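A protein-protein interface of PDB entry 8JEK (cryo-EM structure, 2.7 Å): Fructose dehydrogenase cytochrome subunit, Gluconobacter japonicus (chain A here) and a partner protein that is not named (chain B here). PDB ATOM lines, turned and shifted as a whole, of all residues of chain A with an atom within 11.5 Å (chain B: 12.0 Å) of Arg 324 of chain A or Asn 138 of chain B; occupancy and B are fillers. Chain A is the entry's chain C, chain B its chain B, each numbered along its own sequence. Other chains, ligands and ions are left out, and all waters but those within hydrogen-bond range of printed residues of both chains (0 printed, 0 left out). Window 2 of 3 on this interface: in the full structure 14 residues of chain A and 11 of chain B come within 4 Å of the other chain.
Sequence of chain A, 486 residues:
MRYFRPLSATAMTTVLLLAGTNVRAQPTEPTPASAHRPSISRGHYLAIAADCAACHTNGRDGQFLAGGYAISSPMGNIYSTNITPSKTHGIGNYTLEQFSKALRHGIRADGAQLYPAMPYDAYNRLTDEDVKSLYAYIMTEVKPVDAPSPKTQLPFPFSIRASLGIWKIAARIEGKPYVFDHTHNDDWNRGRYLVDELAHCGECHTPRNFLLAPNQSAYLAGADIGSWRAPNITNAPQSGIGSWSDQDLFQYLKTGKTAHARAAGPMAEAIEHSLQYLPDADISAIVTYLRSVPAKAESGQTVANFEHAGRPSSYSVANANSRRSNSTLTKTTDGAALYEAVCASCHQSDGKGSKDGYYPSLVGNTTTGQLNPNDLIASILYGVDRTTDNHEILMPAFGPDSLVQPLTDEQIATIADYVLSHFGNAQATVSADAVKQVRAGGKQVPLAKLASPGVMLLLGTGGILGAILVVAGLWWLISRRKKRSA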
ATOM      1  N   TYR A 315     -20.044  -6.213 -18.019  1.00  0.00           N
ATOM      2  CA  TYR A 315     -19.001  -5.268 -18.374  1.00  0.00           C
ATOM      3  C   TYR A 315     -18.542  -4.504 -17.132  1.00  0.00           C
ATOM      4  O   TYR A 315     -18.983  -4.770 -16.010  1.00  0.00           O
ATOM      5  CB  TYR A 315     -19.505  -4.335 -19.483  1.00  0.00           C
ATOM      6  CG  TYR A 315     -20.210  -3.080 -19.022  1.00  0.00           C
ATOM      7  CD1 TYR A 315     -21.229  -3.126 -18.079  1.00  0.00           C
ATOM      8  CD2 TYR A 315     -19.867  -1.845 -19.554  1.00  0.00           C
ATOM      9  CE1 TYR A 315     -21.866  -1.974 -17.664  1.00  0.00           C
ATOM     10  CE2 TYR A 315     -20.498  -0.693 -19.149  1.00  0.00           C
ATOM     11  CZ  TYR A 315     -21.497  -0.762 -18.204  1.00  0.00           C
ATOM     12  OH  TYR A 315     -22.132   0.390 -17.802  1.00  0.00           O
ATOM     13  N   SER A 316     -17.649  -3.538 -17.333  1.00  0.00           N
ATOM     14  CA  SER A 316     -17.148  -2.678 -16.269  1.00  0.00           C
ATOM     15  C   SER A 316     -17.487  -1.235 -16.609  1.00  0.00           C
ATOM     16  O   SER A 316     -17.078  -0.730 -17.660  1.00  0.00           O
ATOM     17  CB  SER A 316     -15.638  -2.849 -16.091  1.00  0.00           C
ATOM     18  OG  SER A 316     -15.209  -2.346 -14.839  1.00  0.00           O
ATOM     19  N   VAL A 317     -18.236  -0.578 -15.722  1.00  0.00           N
ATOM     20  CA  VAL A 317     -18.565   0.829 -15.920  1.00  0.00           C
ATOM     21  C   VAL A 317     -17.319   1.694 -15.781  1.00  0.00           C
ATOM     22  O   VAL A 317     -17.140   2.671 -16.517  1.00  0.00           O
ATOM     23  CB  VAL A 317     -19.665   1.265 -14.935  1.00  0.00           C
ATOM     24  CG1 VAL A 317     -20.286   2.579 -15.373  1.00  0.00           C
ATOM     25  CG2 VAL A 317     -20.723   0.188 -14.814  1.00  0.00           C
ATOM     26  N   ALA A 318     -16.441   1.353 -14.834  1.00  0.00           N
ATOM     27  CA  ALA A 318     -15.256   2.169 -14.581  1.00  0.00           C
ATOM     28  C   ALA A 318     -14.344   2.214 -15.800  1.00  0.00           C
ATOM     29  O   ALA A 318     -13.881   3.289 -16.204  1.00  0.00           O
ATOM     30  CB  ALA A 318     -14.505   1.628 -13.366  1.00  0.00           C
ATOM     31  N   ASN A 319     -14.101   1.059 -16.421  1.00  0.00           N
ATOM     32  CA  ASN A 319     -13.202   0.987 -17.566  1.00  0.00           C
ATOM     33  C   ASN A 319     -13.690   1.813 -18.746  1.00  0.00           C
ATOM     34  O   ASN A 319     -12.896   2.099 -19.648  1.00  0.00           O
ATOM     35  CB  ASN A 319     -13.021  -0.466 -18.001  1.00  0.00           C
ATOM     36  CG  ASN A 319     -12.242  -1.282 -16.994  1.00  0.00           C
ATOM     37  OD1 ASN A 319     -11.737  -0.752 -16.005  1.00  0.00           O
ATOM     38  ND2 ASN A 319     -12.137  -2.581 -17.240  1.00  0.00           N
ATOM     39  N   ALA A 320     -14.966   2.193 -18.766  1.00  0.00           N
ATOM     40  CA  ALA A 320     -15.493   3.011 -19.847  1.00  0.00           C
ATOM     41  C   ALA A 320     -15.139   4.483 -19.701  1.00  0.00           C
ATOM     42  O   ALA A 320     -15.268   5.230 -20.676  1.00  0.00           O
ATOM     43  CB  ALA A 320     -17.011   2.856 -19.928  1.00  0.00           C
ATOM     44  N   ASN A 321     -14.694   4.915 -18.518  1.00  0.00           N
ATOM     45  CA  ASN A 321     -14.346   6.320 -18.336  1.00  0.00           C
ATOM     46  C   ASN A 321     -13.186   6.744 -19.223  1.00  0.00           C
ATOM     47  O   ASN A 321     -13.070   7.930 -19.548  1.00  0.00           O
ATOM     48  CB  ASN A 321     -14.007   6.597 -16.873  1.00  0.00           C
ATOM     49  CG  ASN A 321     -15.125   6.216 -15.936  1.00  0.00           C
ATOM     50  OD1 ASN A 321     -16.283   6.555 -16.166  1.00  0.00           O
ATOM     51  ND2 ASN A 321     -14.786   5.511 -14.867  1.00  0.00           N
ATOM     52  N   SER A 322     -12.323   5.807 -19.617  1.00  0.00           N
ATOM     53  CA  SER A 322     -11.247   6.138 -20.543  1.00  0.00           C
ATOM     54  C   SER A 322     -11.781   6.442 -21.935  1.00  0.00           C
ATOM     55  O   SER A 322     -11.151   7.192 -22.687  1.00  0.00           O
ATOM     56  CB  SER A 322     -10.238   4.993 -20.608  1.00  0.00           C
ATOM     57  OG  SER A 322     -10.822   3.835 -21.177  1.00  0.00           O
ATOM     58  N   ARG A 323     -12.930   5.876 -22.294  1.00  0.00           N
ATOM     59  CA  ARG A 323     -13.483   6.040 -23.630  1.00  0.00           C
ATOM     60  C   ARG A 323     -14.390   7.254 -23.756  1.00  0.00           C
ATOM     61  O   ARG A 323     -14.960   7.472 -24.828  1.00  0.00           O
ATOM     62  CB  ARG A 323     -14.241   4.779 -24.049  1.00  0.00           C
ATOM     63  CG  ARG A 323     -13.375   3.787 -24.794  1.00  0.00           C
ATOM     64  CD  ARG A 323     -14.109   2.498 -25.097  1.00  0.00           C
ATOM     65  NE  ARG A 323     -15.066   2.125 -24.064  1.00  0.00           N
ATOM     66  CZ  ARG A 323     -14.856   1.180 -23.161  1.00  0.00           C
ATOM     67  NH1 ARG A 323     -13.712   0.520 -23.104  1.00  0.00           N
ATOM     68  NH2 ARG A 323     -15.821   0.883 -22.297  1.00  0.00           N
ATOM     69  N   ARG A 324     -14.553   8.036 -22.694  1.00  0.00           N
ATOM     70  CA  ARG A 324     -15.211   9.324 -22.834  1.00  0.00           C
ATOM     71  C   ARG A 324     -14.341  10.246 -23.676  1.00  0.00           C
ATOM     72  O   ARG A 324     -13.119  10.085 -23.747  1.00  0.00           O
ATOM     73  CB  ARG A 324     -15.488   9.938 -21.463  1.00  0.00           C
ATOM     74  CG  ARG A 324     -16.333   9.050 -20.565  1.00  0.00           C
ATOM     75  CD  ARG A 324     -16.720   9.752 -19.281  1.00  0.00           C
ATOM     76  NE  ARG A 324     -15.559  10.120 -18.482  1.00  0.00           N
ATOM     77  CZ  ARG A 324     -15.605  10.426 -17.192  1.00  0.00           C
ATOM     78  NH1 ARG A 324     -16.743  10.415 -16.519  1.00  0.00           N
ATOM     79  NH2 ARG A 324     -14.480  10.755 -16.564  1.00  0.00           N
ATOM     80  N   SER A 325     -14.984  11.207 -24.337  1.00  0.00           N
ATOM     81  CA  SER A 325     -14.343  12.067 -25.331  1.00  0.00           C
ATOM     82  C   SER A 325     -13.826  11.275 -26.527  1.00  0.00           C
ATOM     83  O   SER A 325     -12.862  11.687 -27.177  1.00  0.00           O
ATOM     84  CB  SER A 325     -13.208  12.897 -24.720  1.00  0.00           C
ATOM     85  OG  SER A 325     -12.005  12.150 -24.671  1.00  0.00           O
ATOM     86  N   ASN A 326     -14.457  10.142 -26.831  1.00  0.00           N
ATOM     87  CA  ASN A 326     -14.057   9.301 -27.952  1.00  0.00           C
ATOM     88  C   ASN A 326     -15.238   8.991 -28.862  1.00  0.00           C
ATOM     89  O   ASN A 326     -15.525   7.819 -29.122  1.00  0.00           O
ATOM     90  CB  ASN A 326     -13.420   7.995 -27.466  1.00  0.00           C
ATOM     91  CG  ASN A 326     -11.914   8.092 -27.343  1.00  0.00           C
ATOM     92  OD1 ASN A 326     -11.355   7.931 -26.259  1.00  0.00           O
ATOM     93  ND2 ASN A 326     -11.246   8.356 -28.458  1.00  0.00           N
ATOM     94  N   SER A 327     -15.932  10.029 -29.334  1.00  0.00           N
ATOM     95  CA  SER A 327     -17.092   9.888 -30.212  1.00  0.00           C
ATOM     96  C   SER A 327     -16.812   8.958 -31.388  1.00  0.00           C
ATOM     97  O   SER A 327     -15.651   8.729 -31.736  1.00  0.00           O
ATOM     98  CB  SER A 327     -17.533  11.257 -30.734  1.00  0.00           C
ATOM     99  OG  SER A 327     -16.538  11.842 -31.554  1.00  0.00           O
ATOM    100  N   THR A 328     -17.874   8.393 -31.971  1.00  0.00           N
ATOM    101  CA  THR A 328     -17.810   7.433 -33.075  1.00  0.00           C
ATOM    102  C   THR A 328     -16.953   6.221 -32.696  1.00  0.00           C
ATOM    103  O   THR A 328     -15.838   6.033 -33.191  1.00  0.00           O
ATOM    104  CB  THR A 328     -17.416   8.129 -34.407  1.00  0.00           C
ATOM    105  OG1 THR A 328     -17.928   7.375 -35.514  1.00  0.00           O
ATOM    106  CG2 THR A 328     -15.917   8.419 -34.618  1.00  0.00           C
ATOM    107  N   LEU A 329     -17.485   5.397 -31.787  1.00  0.00           N
ATOM    108  CA  LEU A 329     -16.758   4.284 -31.185  1.00  0.00           C
ATOM    109  C   LEU A 329     -15.971   3.452 -32.189  1.00  0.00           C
ATOM    110  O   LEU A 329     -16.537   2.792 -33.065  1.00  0.00           O
ATOM    111  CB  LEU A 329     -17.713   3.369 -30.402  1.00  0.00           C
ATOM    112  CG  LEU A 329     -19.076   2.887 -30.918  1.00  0.00           C
ATOM    113  CD1 LEU A 329     -18.990   1.608 -31.723  1.00  0.00           C
ATOM    114  CD2 LEU A 329     -20.002   2.672 -29.742  1.00  0.00           C
ATOM    115  N   THR A 330     -14.648   3.512 -32.069  1.00  0.00           N
ATOM    116  CA  THR A 330     -13.734   2.598 -32.744  1.00  0.00           C
ATOM    117  C   THR A 330     -12.653   2.064 -31.823  1.00  0.00           C
ATOM    118  O   THR A 330     -11.991   1.085 -32.184  1.00  0.00           O
ATOM    119  CB  THR A 330     -13.071   3.276 -33.949  1.00  0.00           C
ATOM    120  OG1 THR A 330     -12.503   4.527 -33.543  1.00  0.00           O
ATOM    121  CG2 THR A 330     -14.085   3.518 -35.055  1.00  0.00           C
ATOM    122  N   LYS A 331     -12.449   2.667 -30.655  1.00  0.00           N
ATOM    123  CA  LYS A 331     -11.597   2.130 -29.608  1.00  0.00           C
ATOM    124  C   LYS A 331     -12.370   1.264 -28.625  1.00  0.00           C
ATOM    125  O   LYS A 331     -11.787   0.785 -27.648  1.00  0.00           O
ATOM    126  CB  LYS A 331     -10.907   3.273 -28.858  1.00  0.00           C
ATOM    127  CG  LYS A 331     -10.151   4.230 -29.759  1.00  0.00           C
ATOM    128  CD  LYS A 331      -9.469   5.320 -28.956  1.00  0.00           C
ATOM    129  CE  LYS A 331      -8.660   6.240 -29.854  1.00  0.00           C
ATOM    130  NZ  LYS A 331      -9.526   7.018 -30.781  1.00  0.00           N
ATOM    131  N   THR A 332     -13.666   1.065 -28.857  1.00  0.00           N
ATOM    132  CA  THR A 332     -14.504   0.198 -28.033  1.00  0.00           C
ATOM    133  C   THR A 332     -14.494  -1.184 -28.675  1.00  0.00           C
ATOM    134  O   THR A 332     -15.440  -1.582 -29.354  1.00  0.00           O
ATOM    135  CB  THR A 332     -15.919   0.751 -27.915  1.00  0.00           C
ATOM    136  OG1 THR A 332     -15.868   2.171 -27.739  1.00  0.00           O
ATOM    137  CG2 THR A 332     -16.638   0.125 -26.734  1.00  0.00           C
ATOM    138  N   ALA A 337     -18.509  -4.140 -23.469  1.00  0.00           N
ATOM    139  CA  ALA A 337     -18.816  -2.725 -23.640  1.00  0.00           C
ATOM    140  C   ALA A 337     -19.668  -2.492 -24.880  1.00  0.00           C
ATOM    141  O   ALA A 337     -20.582  -1.660 -24.866  1.00  0.00           O
ATOM    142  CB  ALA A 337     -17.524  -1.915 -23.716  1.00  0.00           C
ATOM    143  N   ALA A 341     -23.364  -0.846 -24.902  1.00  0.00           N
ATOM    144  CA  ALA A 341     -23.660   0.387 -25.618  1.00  0.00           C
ATOM    145  C   ALA A 341     -24.755   0.184 -26.657  1.00  0.00           C
ATOM    146  O   ALA A 341     -25.613   1.055 -26.836  1.00  0.00           O
ATOM    147  CB  ALA A 341     -22.391   0.928 -26.273  1.00  0.00           C
ATOM    148  N   ALA B  78      -9.694   3.545  -6.292  1.00  0.00           N
ATOM    149  CA  ALA B  78      -9.757   4.994  -6.459  1.00  0.00           C
ATOM    150  C   ALA B  78      -9.603   5.720  -5.128  1.00  0.00           C
ATOM    151  O   ALA B  78      -8.955   6.771  -5.060  1.00  0.00           O
ATOM    152  CB  ALA B  78     -11.066   5.380  -7.139  1.00  0.00           C
ATOM    153  N   SER B 130     -23.825   7.047  -5.380  1.00  0.00           N
ATOM    154  CA  SER B 130     -23.785   7.866  -6.583  1.00  0.00           C
ATOM    155  C   SER B 130     -22.875   7.329  -7.673  1.00  0.00           C
ATOM    156  O   SER B 130     -23.060   7.681  -8.839  1.00  0.00           O
ATOM    157  CB  SER B 130     -23.347   9.292  -6.235  1.00  0.00           C
ATOM    158  OG  SER B 130     -21.996   9.327  -5.816  1.00  0.00           O
ATOM    159  N   GLY B 131     -21.898   6.493  -7.331  1.00  0.00           N
ATOM    160  CA  GLY B 131     -20.978   5.961  -8.310  1.00  0.00           C
ATOM    161  C   GLY B 131     -19.813   6.860  -8.655  1.00  0.00           C
ATOM    162  O   GLY B 131     -19.026   6.509  -9.541  1.00  0.00           O
ATOM    163  N   VAL B 132     -19.680   8.007  -7.993  1.00  0.00           N
ATOM    164  CA  VAL B 132     -18.562   8.916  -8.199  1.00  0.00           C
ATOM    165  C   VAL B 132     -17.936   9.227  -6.849  1.00  0.00           C
ATOM    166  O   VAL B 132     -18.586   9.136  -5.803  1.00  0.00           O
ATOM    167  CB  VAL B 132     -18.981  10.224  -8.908  1.00  0.00           C
ATOM    168  CG1 VAL B 132     -19.269   9.968 -10.369  1.00  0.00           C
ATOM    169  CG2 VAL B 132     -20.183  10.844  -8.218  1.00  0.00           C
ATOM    170  N   ILE B 133     -16.660   9.602  -6.880  1.00  0.00           N
ATOM    171  CA  ILE B 133     -15.905   9.915  -5.679  1.00  0.00           C
ATOM    172  C   ILE B 133     -15.524  11.389  -5.621  1.00  0.00           C
ATOM    173  O   ILE B 133     -15.598  12.010  -4.560  1.00  0.00           O
ATOM    174  CB  ILE B 133     -14.657   9.015  -5.579  1.00  0.00           C
ATOM    175  CG1 ILE B 133     -15.077   7.546  -5.571  1.00  0.00           C
ATOM    176  CG2 ILE B 133     -13.848   9.352  -4.347  1.00  0.00           C
ATOM    177  CD1 ILE B 133     -13.932   6.587  -5.492  1.00  0.00           C
ATOM    178  N   GLU B 134     -15.126  11.966  -6.750  1.00  0.00           N
ATOM    179  CA  GLU B 134     -14.781  13.376  -6.815  1.00  0.00           C
ATOM    180  C   GLU B 134     -16.054  14.198  -7.013  1.00  0.00           C
ATOM    181  O   GLU B 134     -17.172  13.689  -6.907  1.00  0.00           O
ATOM    182  CB  GLU B 134     -13.757  13.618  -7.921  1.00  0.00           C
ATOM    183  CG  GLU B 134     -12.566  12.683  -7.871  1.00  0.00           C
ATOM    184  CD  GLU B 134     -11.376  13.217  -8.640  1.00  0.00           C
ATOM    185  OE1 GLU B 134     -11.574  13.731  -9.760  1.00  0.00           O
ATOM    186  OE2 GLU B 134     -10.243  13.124  -8.125  1.00  0.00           O
ATOM    187  N   ASP B 135     -15.895  15.492  -7.306  1.00  0.00           N
ATOM    188  CA  ASP B 135     -17.049  16.371  -7.449  1.00  0.00           C
ATOM    189  C   ASP B 135     -16.972  17.234  -8.706  1.00  0.00           C
ATOM    190  O   ASP B 135     -17.573  18.314  -8.740  1.00  0.00           O
ATOM    191  CB  ASP B 135     -17.194  17.266  -6.215  1.00  0.00           C
ATOM    192  CG  ASP B 135     -18.633  17.651  -5.941  1.00  0.00           C
ATOM    193  OD1 ASP B 135     -19.519  17.241  -6.719  1.00  0.00           O
ATOM    194  OD2 ASP B 135     -18.878  18.361  -4.944  1.00  0.00           O
ATOM    195  N   GLU B 136     -16.258  16.791  -9.734  1.00  0.00           N
ATOM    196  CA  GLU B 136     -16.122  17.543 -10.971  1.00  0.00           C
ATOM    197  C   GLU B 136     -16.984  16.927 -12.069  1.00  0.00           C
ATOM    198  O   GLU B 136     -17.604  15.875 -11.899  1.00  0.00           O
ATOM    199  CB  GLU B 136     -14.656  17.594 -11.411  1.00  0.00           C
ATOM    200  CG  GLU B 136     -13.747  18.353 -10.459  1.00  0.00           C
ATOM    201  CD  GLU B 136     -13.216  17.477  -9.344  1.00  0.00           C
ATOM    202  OE1 GLU B 136     -12.913  16.296  -9.611  1.00  0.00           O
ATOM    203  OE2 GLU B 136     -13.100  17.969  -8.202  1.00  0.00           O
ATOM    204  N   THR B 137     -17.014  17.607 -13.215  1.00  0.00           N
ATOM    205  CA  THR B 137     -17.784  17.137 -14.358  1.00  0.00           C
ATOM    206  C   THR B 137     -17.050  16.082 -15.173  1.00  0.00           C
ATOM    207  O   THR B 137     -17.657  15.478 -16.063  1.00  0.00           O
ATOM    208  CB  THR B 137     -18.150  18.313 -15.267  1.00  0.00           C
ATOM    209  OG1 THR B 137     -17.001  18.710 -16.023  1.00  0.00           O
ATOM    210  CG2 THR B 137     -18.634  19.492 -14.436  1.00  0.00           C
ATOM    211  N   ASN B 138     -15.767  15.850 -14.896  1.00  0.00           N
ATOM    212  CA  ASN B 138     -14.993  14.809 -15.559  1.00  0.00           C
ATOM    213  C   ASN B 138     -14.603  13.691 -14.599  1.00  0.00           C
ATOM    214  O   ASN B 138     -13.692  12.913 -14.896  1.00  0.00           O
ATOM    215  CB  ASN B 138     -13.749  15.406 -16.218  1.00  0.00           C
ATOM    216  CG  ASN B 138     -13.019  16.376 -15.312  1.00  0.00           C
ATOM    217  OD1 ASN B 138     -13.569  17.399 -14.904  1.00  0.00           O
ATOM    218  ND2 ASN B 138     -11.770  16.058 -14.992  1.00  0.00           N
ATOM    219  N   ALA B 139     -15.273  13.603 -13.453  1.00  0.00           N
ATOM    220  CA  ALA B 139     -14.973  12.560 -12.485  1.00  0.00           C
ATOM    221  C   ALA B 139     -15.339  11.191 -13.045  1.00  0.00           C
ATOM    222  O   ALA B 139     -16.249  11.051 -13.865  1.00  0.00           O
ATOM    223  CB  ALA B 139     -15.728  12.813 -11.181  1.00  0.00           C
ATOM    224  N   LYS B 140     -14.609  10.173 -12.597  1.00  0.00           N
ATOM    225  CA  LYS B 140     -14.846   8.813 -13.058  1.00  0.00           C
ATOM    226  C   LYS B 140     -16.113   8.260 -12.423  1.00  0.00           C
ATOM    227  O   LYS B 140     -16.300   8.354 -11.206  1.00  0.00           O
ATOM    228  CB  LYS B 140     -13.652   7.920 -12.723  1.00  0.00           C
ATOM    229  CG  LYS B 140     -12.303   8.550 -13.009  1.00  0.00           C
ATOM    230  CD  LYS B 140     -11.946   8.452 -14.480  1.00  0.00           C
ATOM    231  CE  LYS B 140     -11.006   7.286 -14.745  1.00  0.00           C
ATOM    232  NZ  LYS B 140     -10.119   7.537 -15.917  1.00  0.00           N
ATOM    233  N   VAL B 141     -16.981   7.684 -13.249  1.00  0.00           N
ATOM    234  CA  VAL B 141     -18.210   7.048 -12.791  1.00  0.00           C
ATOM    235  C   VAL B 141     -17.944   5.554 -12.678  1.00  0.00           C
ATOM    236  O   VAL B 141     -17.571   4.906 -13.663  1.00  0.00           O
ATOM    237  CB  VAL B 141     -19.382   7.334 -13.743  1.00  0.00           C
ATOM    238  CG1 VAL B 141     -20.595   6.510 -13.356  1.00  0.00           C
ATOM    239  CG2 VAL B 141     -19.725   8.807 -13.727  1.00  0.00           C
ATOM    240  N   TYR B 142     -18.126   5.008 -11.479  1.00  0.00           N
ATOM    241  CA  TYR B 142     -17.857   3.602 -11.223  1.00  0.00           C
ATOM    242  C   TYR B 142     -19.117   2.754 -11.155  1.00  0.00           C
ATOM    243  O   TYR B 142     -19.015   1.522 -11.159  1.00  0.00           O
ATOM    244  CB  TYR B 142     -17.067   3.446  -9.917  1.00  0.00           C
ATOM    245  CG  TYR B 142     -15.786   4.247  -9.894  1.00  0.00           C
ATOM    246  CD1 TYR B 142     -14.660   3.811 -10.576  1.00  0.00           C
ATOM    247  CD2 TYR B 142     -15.707   5.445  -9.201  1.00  0.00           C
ATOM    248  CE1 TYR B 142     -13.493   4.541 -10.566  1.00  0.00           C
ATOM    249  CE2 TYR B 142     -14.543   6.181  -9.183  1.00  0.00           C
ATOM    250  CZ  TYR B 142     -13.439   5.724  -9.867  1.00  0.00           C
ATOM    251  OH  TYR B 142     -12.276   6.456  -9.855  1.00  0.00           O
ATOM    252  N   ALA B 143     -20.294   3.371 -11.098  1.00  0.00           N
ATOM    253  CA  ALA B 143     -21.541   2.621 -11.003  1.00  0.00           C
ATOM    254  C   ALA B 143     -22.676   3.482 -11.527  1.00  0.00           C
ATOM    255  O   ALA B 143     -23.029   4.486 -10.903  1.00  0.00           O
ATOM    256  CB  ALA B 143     -21.812   2.192  -9.563  1.00  0.00           C
ATOM    257  N   PHE B 144     -23.232   3.102 -12.671  1.00  0.00           N
ATOM    258  CA  PHE B 144     -24.491   3.638 -13.161  1.00  0.00           C
ATOM    259  C   PHE B 144     -25.433   2.475 -13.422  1.00  0.00           C
ATOM    260  O   PHE B 144     -25.019   1.442 -13.958  1.00  0.00           O
ATOM    261  CB  PHE B 144     -24.305   4.461 -14.436  1.00  0.00           C
ATOM    262  CG  PHE B 144     -25.597   4.913 -15.053  1.00  0.00           C
ATOM    263  CD1 PHE B 144     -26.422   5.804 -14.389  1.00  0.00           C
ATOM    264  CD2 PHE B 144     -25.993   4.439 -16.287  1.00  0.00           C
ATOM    265  CE1 PHE B 144     -27.612   6.217 -14.951  1.00  0.00           C
ATOM    266  CE2 PHE B 144     -27.180   4.849 -16.850  1.00  0.00           C
ATOM    267  CZ  PHE B 144     -27.989   5.740 -16.180  1.00  0.00           C
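The backbone carbonyl oxygen (O) of Asn 321 of chain A lies within hydrogen-bond range of the guanidinium group (NE) of Arg 324 of chain A (3.5 Å). O of Ala 318 of chain A lies within hydrogen-bond range of ND2 of Asn 321 of chain A (2.7 Å). The backbone carbonyl oxygen of Gly 131 of chain B sits at hydrogen-bond distance from the backbone NH of Tyr 142 of chain B (2.6 Å).
NH2 of Arg 324 of chain A is in hydrogen-bond range of O of Asn 138 of chain B, 2.8 Å away. The backbone carbonyl oxygen of Ala 139 of chain B is in hydrogen-bond range of the guanidinium group of Arg 324 of chain A, at 2.8 Å. The side-chain amide nitrogen (ND2) of Asn 321 of chain A is in hydrogen-bond range of the backbone carbonyl oxygen (O) of Val 141 of chain B (3.1 Å).
Of the 16 printed residues of chain B, 5 touch a printed residue of chain A. Printed residues of chain B that touch a printed residue of chain A: Asn 138, Ala 139, Lys 140, Val 141 and Tyr 142. Hydrophobic or aromatic side chains of chain B that line the printed part of chain A: Tyr 142. Hydrophobic or aromatic side chains of chain A that line the printed part of chain B: Val 317 and Ala 318.
Among the printed residues, merely in contact across the chains: Asn 321 of chain A with Lys 140 of chain B (3.4 Å), Ala 318 of chain A with Tyr 142 of chain B (3.5 Å), Val 317 of chain A with Val 141 of chain B (3.7 Å), Ala 318 of chain A with Val 141 of chain B (3.7 Å) and Val 317 of chain A with Tyr 142 of chain B (3.8 Å).
Of the printed residues of chain B, Val 317 of chain A touches Val 141 (3.7 Å) and Tyr 142 (3.8 Å). Of the printed residues of chain B, Ala 318 of chain A touches Val 141 and Tyr 142. Ala 320 of chain A touches none of the printed residues of chain B. No residue of chain B comes within 4 Å of Arg 323 of chain A. Of the printed residues of chain B, Arg 324 of chain A touches Asn 138 (2.8 Å) and Ala 139 (2.8 Å). No residue of chain B comes within 4 Å of Asn 326 of chain A. Ser 327 of chain A touches none of the printed residues of chain B. Gly 131 of chain B touches none of the printed residues of chain A. No residue of chain A comes within 4 Å of Glu 136 of chain B. No residue of chain A comes within 4 Å of Thr 137 of chain B. Asn 138 of chain B touches one residue of chain A. Of the printed residues of chain A, Lys 140 of chain B touches Asn 321. Of chain A, only Val 317, Ala 318 and Asn 321 come within 4 Å of Val 141 of chain B. Of the printed residues of chain A, Tyr 142 of chain B touches Val 317 (3.8 Å) and Ala 318 (3.5 Å). The nearest printed residue of chain A that does not touch Tyr 142 of chain B is Asn 321 of chain A (4.6 Å).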
